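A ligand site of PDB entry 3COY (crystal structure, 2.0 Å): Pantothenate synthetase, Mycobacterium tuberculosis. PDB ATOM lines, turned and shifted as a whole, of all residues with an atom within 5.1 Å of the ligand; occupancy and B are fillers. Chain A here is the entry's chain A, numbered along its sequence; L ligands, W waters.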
ATOM      1  N   PRO A  39     -20.031   5.490   3.674  1.00  0.00           N
ATOM      2  CA  PRO A  39     -21.019   5.779   2.608  1.00  0.00           C
ATOM      3  C   PRO A  39     -21.858   7.001   2.924  1.00  0.00           C
ATOM      4  O   PRO A  39     -22.439   7.084   4.010  1.00  0.00           O
ATOM      5  CB  PRO A  39     -21.921   4.526   2.605  1.00  0.00           C
ATOM      6  CG  PRO A  39     -21.015   3.403   3.250  1.00  0.00           C
ATOM      7  CD  PRO A  39     -20.291   4.198   4.338  1.00  0.00           C
ATOM      8  N   THR A  40     -21.893   7.959   2.000  1.00  0.00           N
ATOM      9  CA  THR A  40     -22.805   9.115   2.123  1.00  0.00           C
ATOM     10  C   THR A  40     -23.510   9.484   0.796  1.00  0.00           C
ATOM     11  O   THR A  40     -23.124   9.032  -0.281  1.00  0.00           O
ATOM     12  CB  THR A  40     -22.056  10.379   2.567  1.00  0.00           C
ATOM     13  OG1 THR A  40     -21.397  10.953   1.440  1.00  0.00           O
ATOM     14  CG2 THR A  40     -21.036  10.046   3.657  1.00  0.00           C
ATOM     15  N   MET A  41     -24.540  10.307   0.909  1.00  0.00           N
ATOM     16  CA  MET A  41     -25.179  10.881  -0.280  1.00  0.00           C
ATOM     17  C   MET A  41     -24.723  12.306  -0.483  1.00  0.00           C
ATOM     18  O   MET A  41     -25.305  13.049  -1.263  1.00  0.00           O
ATOM     19  CB  MET A  41     -26.724  10.810  -0.165  1.00  0.00           C
ATOM     20  CG  MET A  41     -27.209   9.393  -0.207  1.00  0.00           C
ATOM     21  SD  MET A  41     -28.973   9.150  -0.532  1.00  0.00           S
ATOM     22  CE  MET A  41     -29.628   9.988   0.882  1.00  0.00           C
ATOM     23  N   GLY A  42     -23.633  12.665   0.182  1.00  0.00           N
ATOM     24  CA  GLY A  42     -23.130  14.046   0.175  1.00  0.00           C
ATOM     25  C   GLY A  42     -23.998  15.001   0.990  1.00  0.00           C
ATOM     26  O   GLY A  42     -24.796  14.574   1.833  1.00  0.00           O
ATOM     27  N   HIS A  45     -22.714  17.328   6.665  1.00  0.00           N
ATOM     28  CA  HIS A  45     -22.853  18.170   7.823  1.00  0.00           C
ATOM     29  C   HIS A  45     -22.187  17.443   8.993  1.00  0.00           C
ATOM     30  O   HIS A  45     -21.616  16.350   8.826  1.00  0.00           O
ATOM     31  CB  HIS A  45     -24.334  18.489   8.089  1.00  0.00           C
ATOM     32  CG  HIS A  45     -25.207  17.276   8.234  1.00  0.00           C
ATOM     33  ND1 HIS A  45     -25.024  16.338   9.226  1.00  0.00           N
ATOM     34  CD2 HIS A  45     -26.284  16.873   7.526  1.00  0.00           C
ATOM     35  CE1 HIS A  45     -25.934  15.390   9.101  1.00  0.00           C
ATOM     36  NE2 HIS A  45     -26.716  15.693   8.083  1.00  0.00           N
ATOM     37  N   GLY A  47     -23.056  15.665  11.364  1.00  0.00           N
ATOM     38  CA  GLY A  47     -23.454  14.273  11.570  1.00  0.00           C
ATOM     39  C   GLY A  47     -22.649  13.306  10.716  1.00  0.00           C
ATOM     40  O   GLY A  47     -22.162  12.289  11.202  1.00  0.00           O
ATOM     41  N   HIS A  48     -22.490  13.613   9.429  1.00  0.00           N
ATOM     42  CA  HIS A  48     -21.651  12.797   8.561  1.00  0.00           C
ATOM     43  C   HIS A  48     -20.211  12.857   9.034  1.00  0.00           C
ATOM     44  O   HIS A  48     -19.496  11.838   8.962  1.00  0.00           O
ATOM     45  CB  HIS A  48     -21.705  13.273   7.114  1.00  0.00           C
ATOM     46  CG  HIS A  48     -23.089  13.341   6.537  1.00  0.00           C
ATOM     47  ND1 HIS A  48     -23.719  14.539   6.283  1.00  0.00           N
ATOM     48  CD2 HIS A  48     -23.938  12.368   6.151  1.00  0.00           C
ATOM     49  CE1 HIS A  48     -24.902  14.297   5.760  1.00  0.00           C
ATOM     50  NE2 HIS A  48     -25.071  12.994   5.666  1.00  0.00           N
ATOM     51  N   LEU A  51     -18.970  10.314  11.584  1.00  0.00           N
ATOM     52  CA  LEU A  51     -18.602   9.002  11.070  1.00  0.00           C
ATOM     53  C   LEU A  51     -17.204   9.070  10.479  1.00  0.00           C
ATOM     54  O   LEU A  51     -16.416   8.145  10.651  1.00  0.00           O
ATOM     55  CB  LEU A  51     -19.556   8.460  10.004  1.00  0.00           C
ATOM     56  CG  LEU A  51     -21.083   8.616   9.972  1.00  0.00           C
ATOM     57  CD1 LEU A  51     -21.698   7.486   9.146  1.00  0.00           C
ATOM     58  CD2 LEU A  51     -21.728   8.730  11.304  1.00  0.00           C
ATOM     59  N   PHE A  68     -22.616   9.456  -3.355  1.00  0.00           N
ATOM     60  CA  PHE A  68     -23.445   8.914  -4.434  1.00  0.00           C
ATOM     61  C   PHE A  68     -24.891   8.950  -4.025  1.00  0.00           C
ATOM     62  O   PHE A  68     -25.252   8.545  -2.911  1.00  0.00           O
ATOM     63  CB  PHE A  68     -23.025   7.457  -4.767  1.00  0.00           C
ATOM     64  CG  PHE A  68     -23.813   6.826  -5.899  1.00  0.00           C
ATOM     65  CD1 PHE A  68     -23.637   7.237  -7.209  1.00  0.00           C
ATOM     66  CD2 PHE A  68     -24.723   5.798  -5.639  1.00  0.00           C
ATOM     67  CE1 PHE A  68     -24.353   6.643  -8.248  1.00  0.00           C
ATOM     68  CE2 PHE A  68     -25.435   5.177  -6.698  1.00  0.00           C
ATOM     69  CZ  PHE A  68     -25.263   5.596  -7.977  1.00  0.00           C
ATOM     70  N   GLN A  73     -33.086   3.700  -4.240  1.00  0.00           N
ATOM     71  CA  GLN A  73     -33.728   3.846  -2.915  1.00  0.00           C
ATOM     72  C   GLN A  73     -34.801   4.950  -2.818  1.00  0.00           C
ATOM     73  O   GLN A  73     -35.400   5.158  -1.754  1.00  0.00           O
ATOM     74  CB  GLN A  73     -32.662   3.971  -1.802  1.00  0.00           C
ATOM     75  CG  GLN A  73     -31.824   5.266  -1.833  1.00  0.00           C
ATOM     76  CD  GLN A  73     -30.611   5.217  -0.911  1.00  0.00           C
ATOM     77  OE1 GLN A  73     -30.540   5.946   0.092  1.00  0.00           O
ATOM     78  NE2 GLN A  73     -29.646   4.364  -1.235  1.00  0.00           N
ATOM     79  N   TYR A  83     -33.100  15.503  -3.605  1.00  0.00           N
ATOM     80  CA  TYR A  83     -32.022  15.569  -2.609  1.00  0.00           C
ATOM     81  C   TYR A  83     -31.028  16.707  -2.885  1.00  0.00           C
ATOM     82  O   TYR A  83     -30.607  16.896  -4.029  1.00  0.00           O
ATOM     83  CB  TYR A  83     -31.298  14.214  -2.521  1.00  0.00           C
ATOM     84  CG  TYR A  83     -30.466  14.054  -1.262  1.00  0.00           C
ATOM     85  CD1 TYR A  83     -31.068  13.683  -0.053  1.00  0.00           C
ATOM     86  CD2 TYR A  83     -29.095  14.315  -1.276  1.00  0.00           C
ATOM     87  CE1 TYR A  83     -30.313  13.556   1.119  1.00  0.00           C
ATOM     88  CE2 TYR A  83     -28.331  14.184  -0.102  1.00  0.00           C
ATOM     89  CZ  TYR A  83     -28.943  13.808   1.088  1.00  0.00           C
ATOM     90  OH  TYR A  83     -28.192  13.682   2.237  1.00  0.00           O
ATOM     91  N   VAL A 140     -30.969   0.585  -0.765  1.00  0.00           N
ATOM     92  CA  VAL A 140     -29.879   0.826   0.169  1.00  0.00           C
ATOM     93  C   VAL A 140     -28.934  -0.365   0.224  1.00  0.00           C
ATOM     94  O   VAL A 140     -27.720  -0.206   0.028  1.00  0.00           O
ATOM     95  CB  VAL A 140     -30.450   1.151   1.568  1.00  0.00           C
ATOM     96  CG1 VAL A 140     -29.344   1.186   2.626  1.00  0.00           C
ATOM     97  CG2 VAL A 140     -31.213   2.488   1.523  1.00  0.00           C
ATOM     98  N   VAL A 143     -26.967  -0.845  -3.092  1.00  0.00           N
ATOM     99  CA  VAL A 143     -25.850   0.075  -3.294  1.00  0.00           C
ATOM    100  C   VAL A 143     -24.720  -0.139  -2.271  1.00  0.00           C
ATOM    101  O   VAL A 143     -23.544  -0.041  -2.616  1.00  0.00           O
ATOM    102  CB  VAL A 143     -26.289   1.566  -3.448  1.00  0.00           C
ATOM    103  CG1 VAL A 143     -26.621   2.227  -2.075  1.00  0.00           C
ATOM    104  CG2 VAL A 143     -25.226   2.375  -4.205  1.00  0.00           C
ATOM    105  N   VAL A 144     -25.067  -0.492  -1.026  1.00  0.00           N
ATOM    106  CA  VAL A 144     -24.032  -0.641  -0.003  1.00  0.00           C
ATOM    107  C   VAL A 144     -23.214  -1.893  -0.279  1.00  0.00           C
ATOM    108  O   VAL A 144     -21.987  -1.901  -0.121  1.00  0.00           O
ATOM    109  CB  VAL A 144     -24.608  -0.669   1.440  1.00  0.00           C
ATOM    110  CG1 VAL A 144     -23.521  -1.136   2.421  1.00  0.00           C
ATOM    111  CG2 VAL A 144     -25.125   0.703   1.843  1.00  0.00           C
ATOM    112  N   PHE A 157     -18.833   2.447   8.290  1.00  0.00           N
ATOM    113  CA  PHE A 157     -19.443   3.291   9.324  1.00  0.00           C
ATOM    114  C   PHE A 157     -20.868   3.769   8.967  1.00  0.00           C
ATOM    115  O   PHE A 157     -21.102   4.262   7.854  1.00  0.00           O
ATOM    116  CB  PHE A 157     -18.507   4.480   9.591  1.00  0.00           C
ATOM    117  CG  PHE A 157     -17.204   4.049  10.186  1.00  0.00           C
ATOM    118  CD1 PHE A 157     -16.236   3.401   9.407  1.00  0.00           C
ATOM    119  CD2 PHE A 157     -16.991   4.186  11.547  1.00  0.00           C
ATOM    120  CE1 PHE A 157     -15.033   2.953   9.965  1.00  0.00           C
ATOM    121  CE2 PHE A 157     -15.774   3.752  12.120  1.00  0.00           C
ATOM    122  CZ  PHE A 157     -14.819   3.119  11.333  1.00  0.00           C
ATOM    123  N   PHE A 158     -21.792   3.590   9.902  1.00  0.00           N
ATOM    124  CA  PHE A 158     -23.180   4.056   9.745  1.00  0.00           C
ATOM    125  C   PHE A 158     -23.693   4.795  10.985  1.00  0.00           C
ATOM    126  O   PHE A 158     -23.383   4.400  12.101  1.00  0.00           O
ATOM    127  CB  PHE A 158     -24.094   2.867   9.432  1.00  0.00           C
ATOM    128  CG  PHE A 158     -23.979   2.391   7.993  1.00  0.00           C
ATOM    129  CD1 PHE A 158     -23.088   1.376   7.644  1.00  0.00           C
ATOM    130  CD2 PHE A 158     -24.736   2.995   6.993  1.00  0.00           C
ATOM    131  CE1 PHE A 158     -22.968   0.970   6.315  1.00  0.00           C
ATOM    132  CE2 PHE A 158     -24.616   2.575   5.638  1.00  0.00           C
ATOM    133  CZ  PHE A 158     -23.743   1.587   5.320  1.00  0.00           C
ATOM    134  N   GLY A 159     -24.490   5.846  10.801  1.00  0.00           N
ATOM    135  CA  GLY A 159     -25.013   6.599  11.965  1.00  0.00           C
ATOM    136  C   GLY A 159     -26.195   5.919  12.606  1.00  0.00           C
ATOM    137  O   GLY A 159     -27.025   5.342  11.900  1.00  0.00           O
ATOM    138  N   GLU A 160     -26.312   5.968  13.936  1.00  0.00           N
ATOM    139  CA  GLU A 160     -27.522   5.475  14.612  1.00  0.00           C
ATOM    140  C   GLU A 160     -28.763   6.316  14.271  1.00  0.00           C
ATOM    141  O   GLU A 160     -29.897   5.929  14.570  1.00  0.00           O
ATOM    142  CB  GLU A 160     -27.333   5.436  16.138  1.00  0.00           C
ATOM    143  CG  GLU A 160     -26.477   4.267  16.626  1.00  0.00           C
ATOM    144  CD  GLU A 160     -26.120   4.410  18.096  1.00  0.00           C
ATOM    145  OE1 GLU A 160     -26.777   5.222  18.795  1.00  0.00           O
ATOM    146  OE2 GLU A 160     -25.166   3.729  18.533  1.00  0.00           O
ATOM    147  N   LYS A 161     -28.524   7.466  13.674  1.00  0.00           N
ATOM    148  CA  LYS A 161     -29.543   8.370  13.161  1.00  0.00           C
ATOM    149  C   LYS A 161     -30.515   7.572  12.280  1.00  0.00           C
ATOM    150  O   LYS A 161     -31.744   7.634  12.424  1.00  0.00           O
ATOM    151  CB  LYS A 161     -28.835   9.442  12.364  1.00  0.00           C
ATOM    152  CG  LYS A 161     -29.427  10.803  12.488  1.00  0.00           C
ATOM    153  CD  LYS A 161     -30.537  10.945  11.538  1.00  0.00           C
ATOM    154  CE  LYS A 161     -31.244  12.237  11.746  1.00  0.00           C
ATOM    155  NZ  LYS A 161     -32.616  12.017  11.212  1.00  0.00           N
ATOM    156  N   ASP A 162     -29.953   6.768  11.384  1.00  0.00           N
ATOM    157  CA  ASP A 162     -30.764   5.906  10.549  1.00  0.00           C
ATOM    158  C   ASP A 162     -30.652   4.495  11.117  1.00  0.00           C
ATOM    159  O   ASP A 162     -29.966   3.626  10.575  1.00  0.00           O
ATOM    160  CB  ASP A 162     -30.287   6.044   9.114  1.00  0.00           C
ATOM    161  CG  ASP A 162     -30.438   7.457   8.625  1.00  0.00           C
ATOM    162  OD1 ASP A 162     -31.577   7.789   8.199  1.00  0.00           O
ATOM    163  OD2 ASP A 162     -29.478   8.258   8.695  1.00  0.00           O
ATOM    164  N   GLN A 165     -31.760   1.354   9.024  1.00  0.00           N
ATOM    165  CA  GLN A 165     -30.722   1.163   8.017  1.00  0.00           C
ATOM    166  C   GLN A 165     -29.493   0.452   8.606  1.00  0.00           C
ATOM    167  O   GLN A 165     -28.999  -0.495   8.028  1.00  0.00           O
ATOM    168  CB  GLN A 165     -30.305   2.509   7.448  1.00  0.00           C
ATOM    169  CG  GLN A 165     -29.060   2.478   6.615  1.00  0.00           C
ATOM    170  CD  GLN A 165     -28.873   3.777   5.891  1.00  0.00           C
ATOM    171  OE1 GLN A 165     -29.431   3.971   4.807  1.00  0.00           O
ATOM    172  NE2 GLN A 165     -28.110   4.684   6.484  1.00  0.00           N
ATOM    173  N   VAL A 185     -22.403   4.745  14.723  1.00  0.00           N
ATOM    174  CA  VAL A 185     -21.880   5.968  15.305  1.00  0.00           C
ATOM    175  C   VAL A 185     -23.070   6.716  15.927  1.00  0.00           C
ATOM    176  O   VAL A 185     -24.137   6.839  15.284  1.00  0.00           O
ATOM    177  CB  VAL A 185     -21.101   6.778  14.241  1.00  0.00           C
ATOM    178  CG1 VAL A 185     -20.453   8.051  14.806  1.00  0.00           C
ATOM    179  CG2 VAL A 185     -20.031   5.921  13.645  1.00  0.00           C
ATOM    180  N   PRO A 186     -22.932   7.177  17.202  1.00  0.00           N
ATOM    181  CA  PRO A 186     -24.009   7.921  17.860  1.00  0.00           C
ATOM    182  C   PRO A 186     -24.506   9.138  17.059  1.00  0.00           C
ATOM    183  O   PRO A 186     -23.709   9.797  16.363  1.00  0.00           O
ATOM    184  CB  PRO A 186     -23.370   8.382  19.178  1.00  0.00           C
ATOM    185  CG  PRO A 186     -22.321   7.335  19.438  1.00  0.00           C
ATOM    186  CD  PRO A 186     -21.759   7.014  18.084  1.00  0.00           C
ATOM    187  N   THR A 187     -25.813   9.422  17.184  1.00  0.00           N
ATOM    188  CA  THR A 187     -26.491  10.531  16.488  1.00  0.00           C
ATOM    189  C   THR A 187     -25.935  11.891  16.937  1.00  0.00           C
ATOM    190  O   THR A 187     -25.890  12.198  18.137  1.00  0.00           O
ATOM    191  CB  THR A 187     -28.023  10.483  16.728  1.00  0.00           C
ATOM    192  OG1 THR A 187     -28.564   9.277  16.160  1.00  0.00           O
ATOM    193  CG2 THR A 187     -28.737  11.675  16.101  1.00  0.00           C
ATOM    194  N   VAL A 188     -25.504  12.703  15.988  1.00  0.00           N
ATOM    195  CA  VAL A 188     -25.038  14.045  16.311  1.00  0.00           C
ATOM    196  C   VAL A 188     -26.244  14.957  16.341  1.00  0.00           C
ATOM    197  O   VAL A 188     -27.076  14.912  15.424  1.00  0.00           O
ATOM    198  CB  VAL A 188     -23.992  14.570  15.299  1.00  0.00           C
ATOM    199  CG1 VAL A 188     -23.531  16.001  15.664  1.00  0.00           C
ATOM    200  CG2 VAL A 188     -22.822  13.648  15.262  1.00  0.00           C
ATOM    201  N   ALA A 195     -31.941  16.153  16.080  1.00  0.00           N
ATOM    202  CA  ALA A 195     -31.016  15.290  15.328  1.00  0.00           C
ATOM    203  C   ALA A 195     -30.632  15.992  14.041  1.00  0.00           C
ATOM    204  O   ALA A 195     -31.506  16.353  13.243  1.00  0.00           O
ATOM    205  CB  ALA A 195     -31.633  13.945  15.031  1.00  0.00           C
ATOM    206  N   MET A 196     -29.334  16.179  13.818  1.00  0.00           N
ATOM    207  CA  MET A 196     -28.841  16.810  12.602  1.00  0.00           C
ATOM    208  C   MET A 196     -29.191  15.996  11.351  1.00  0.00           C
ATOM    209  O   MET A 196     -28.905  14.790  11.246  1.00  0.00           O
ATOM    210  CB  MET A 196     -27.340  17.054  12.666  1.00  0.00           C
ATOM    211  CG  MET A 196     -26.952  18.384  13.212  1.00  0.00           C
ATOM    212  SD  MET A 196     -25.155  18.541  13.277  1.00  0.00           S
ATOM    213  CE  MET A 196     -24.994  19.867  14.464  1.00  0.00           C
ATOM    214  N   SER A 197     -29.828  16.680  10.409  1.00  0.00           N
ATOM    215  CA  SER A 197     -30.224  16.091   9.149  1.00  0.00           C
ATOM    216  C   SER A 197     -30.213  17.233   8.124  1.00  0.00           C
ATOM    217  O   SER A 197     -30.452  18.393   8.470  1.00  0.00           O
ATOM    218  CB  SER A 197     -31.641  15.513   9.256  1.00  0.00           C
ATOM    219  OG  SER A 197     -32.050  14.895   8.046  1.00  0.00           O
HETATM  220  C1  LIG L   1     -27.456   7.422   3.498  1.00  0.00           C
HETATM  221  C2  LIG L   1     -24.906  10.525  13.096  1.00  0.00           C
HETATM  222  C3  LIG L   1     -27.646   6.394   2.408  1.00  0.00           C
HETATM  223  C4  LIG L   1     -25.613  10.641  10.869  1.00  0.00           C
HETATM  224  C5  LIG L   1     -26.323  11.818  11.118  1.00  0.00           C
HETATM  225  C6  LIG L   1     -26.310  12.328  12.400  1.00  0.00           C
HETATM  226  C7  LIG L   1     -26.442   5.479   2.094  1.00  0.00           C
HETATM  227  N1  LIG L   1     -25.592  11.658  13.357  1.00  0.00           N
HETATM  228  N2  LIG L   1     -26.924   8.626   3.131  1.00  0.00           N
HETATM  229  O1  LIG L   1     -27.827   7.167   4.643  1.00  0.00           O
HETATM  230  C8  LIG L   1     -26.589  11.289   9.014  1.00  0.00           C
HETATM  231  O2  LIG L   1     -26.965   7.456   9.372  1.00  0.00           O
HETATM  232  N3  LIG L   1     -24.909  10.011  11.861  1.00  0.00           N
HETATM  233  C9  LIG L   1     -26.021   4.691   3.299  1.00  0.00           C
HETATM  234  C10 LIG L   1     -26.856   4.483   1.023  1.00  0.00           C
HETATM  235  C11 LIG L   1     -25.229   6.237   1.558  1.00  0.00           C
HETATM  236  N4  LIG L   1     -28.902   5.548   2.628  1.00  0.00           N
HETATM  237  S1  LIG L   1     -26.702   9.845   4.047  1.00  0.00           S
HETATM  238  O3  LIG L   1     -27.969  10.403   4.409  1.00  0.00           O
HETATM  239  O4  LIG L   1     -25.812  10.796   3.442  1.00  0.00           O
HETATM  240  O5  LIG L   1     -26.023   9.472   5.480  1.00  0.00           O
HETATM  241  C12 LIG L   1     -24.690   8.928   5.486  1.00  0.00           C
HETATM  242  C13 LIG L   1     -24.439   8.387   6.876  1.00  0.00           C
HETATM  243  C14 LIG L   1     -25.571   7.454   7.314  1.00  0.00           C
HETATM  244  O6  LIG L   1     -25.024   6.308   7.927  1.00  0.00           O
HETATM  245  C15 LIG L   1     -26.324   8.256   8.360  1.00  0.00           C
HETATM  246  C16 LIG L   1     -25.226   9.152   8.924  1.00  0.00           C
HETATM  247  O7  LIG L   1     -24.448   9.506   7.791  1.00  0.00           O
HETATM  248  N5  LIG L   1     -25.802  10.343   9.586  1.00  0.00           N
HETATM  249  N6  LIG L   1     -26.923  12.210   9.959  1.00  0.00           N
HETATM  250  N7  LIG L   1     -27.005  13.459  12.696  1.00  0.00           N
HETATM  251  O   HOH W   1     -27.452   4.139   9.288  1.00  0.00           O
HETATM  252  O   HOH W   2     -29.328  10.369   7.172  1.00  0.00           O
HETATM  253  O   HOH W   3     -22.986   5.582   6.216  1.00  0.00           O
HETATM  254  O   HOH W   4     -31.039   7.795   4.167  1.00  0.00           O
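The side-chain carboxylate (OD2) of Asp 162 is in hydrogen-bond range of an oxygen (O2) of the ligand, at 2.7 Å. O of Met 196 lies within hydrogen-bond range of N7 of the ligand (2.7 Å). N4 of the ligand is in hydrogen-bond range of OE1 of Gln 165, at 2.7 Å. A nitrogen (N1) of the ligand sits at hydrogen-bond distance from the backbone NH of Val 188 (2.8 Å). The backbone carbonyl oxygen (O) of Val 188 is in hydrogen-bond range of a nitrogen (N7) of the ligand. The backbone NH (N) of Met 41 lies within hydrogen-bond range of an oxygen (O4) of the ligand (2.9 Å). The backbone NH of Gly 159 sits at hydrogen-bond distance from an oxygen (O6) of the ligand (3.0 Å). The backbone carbonyl oxygen (O) of Gly 159 lies within hydrogen-bond range of an oxygen (O2) of the ligand (3.3 Å). A nitrogen (N4) of the ligand lies within hydrogen-bond range of the side-chain amide oxygen of Gln 73. NE2 of His 48 is in hydrogen-bond range of O4 of the ligand (3.2 Å).
The backbone NH (N) of Met 196 sits at hydrogen-bond distance from the backbone carbonyl oxygen (O) of Val 188. SD of Met 41 sits close to OE1 of Gln 73 (3.6 Å). The backbone NH (N) of His 45 sits at hydrogen-bond distance from a ring nitrogen (ND1) of His 48 (3.0 Å). The backbone carbonyl oxygen (O) of Phe 158 sits at hydrogen-bond distance from the backbone NH (N) of Val 185, 2.8 Å away. A ring nitrogen (ND1) of His 45 lies within hydrogen-bond range of the backbone NH (N) of Gly 47 (3.0 Å). The side-chain hydroxyl (OG1) of Thr 187 is in hydrogen-bond range of the backbone NH (N) of Lys 161, at 3.1 Å. N of Gly 42 sits at hydrogen-bond distance from OG1 of Thr 40 (3.1 Å). The backbone carbonyl oxygen (O) of Thr 40 lies within hydrogen-bond range of the backbone NH (N) of Phe 68 (3.1 Å).
Merely in contact with the ligand: Pro 39, Thr 40, His 45, Gly 47, Leu 51, Tyr 83, Val 140, Val 143, Phe 158, Lys 161, Pro 186 and Thr 187.
Water W3 lies within hydrogen-bond range of O of Pro 39, O6 of the ligand and O of Phe 157. Water W2 bridges the side-chain carboxylate of Asp 162 (2.6 Å) and an oxygen (O3) of the ligand (3.1 Å). Water W1 lies within hydrogen-bond range of O of Asp 162 (2.9 Å), O of Gly 159 (2.9 Å), NE2 of Gln 165 (2.9 Å) and O2 of the ligand (3.4 Å).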
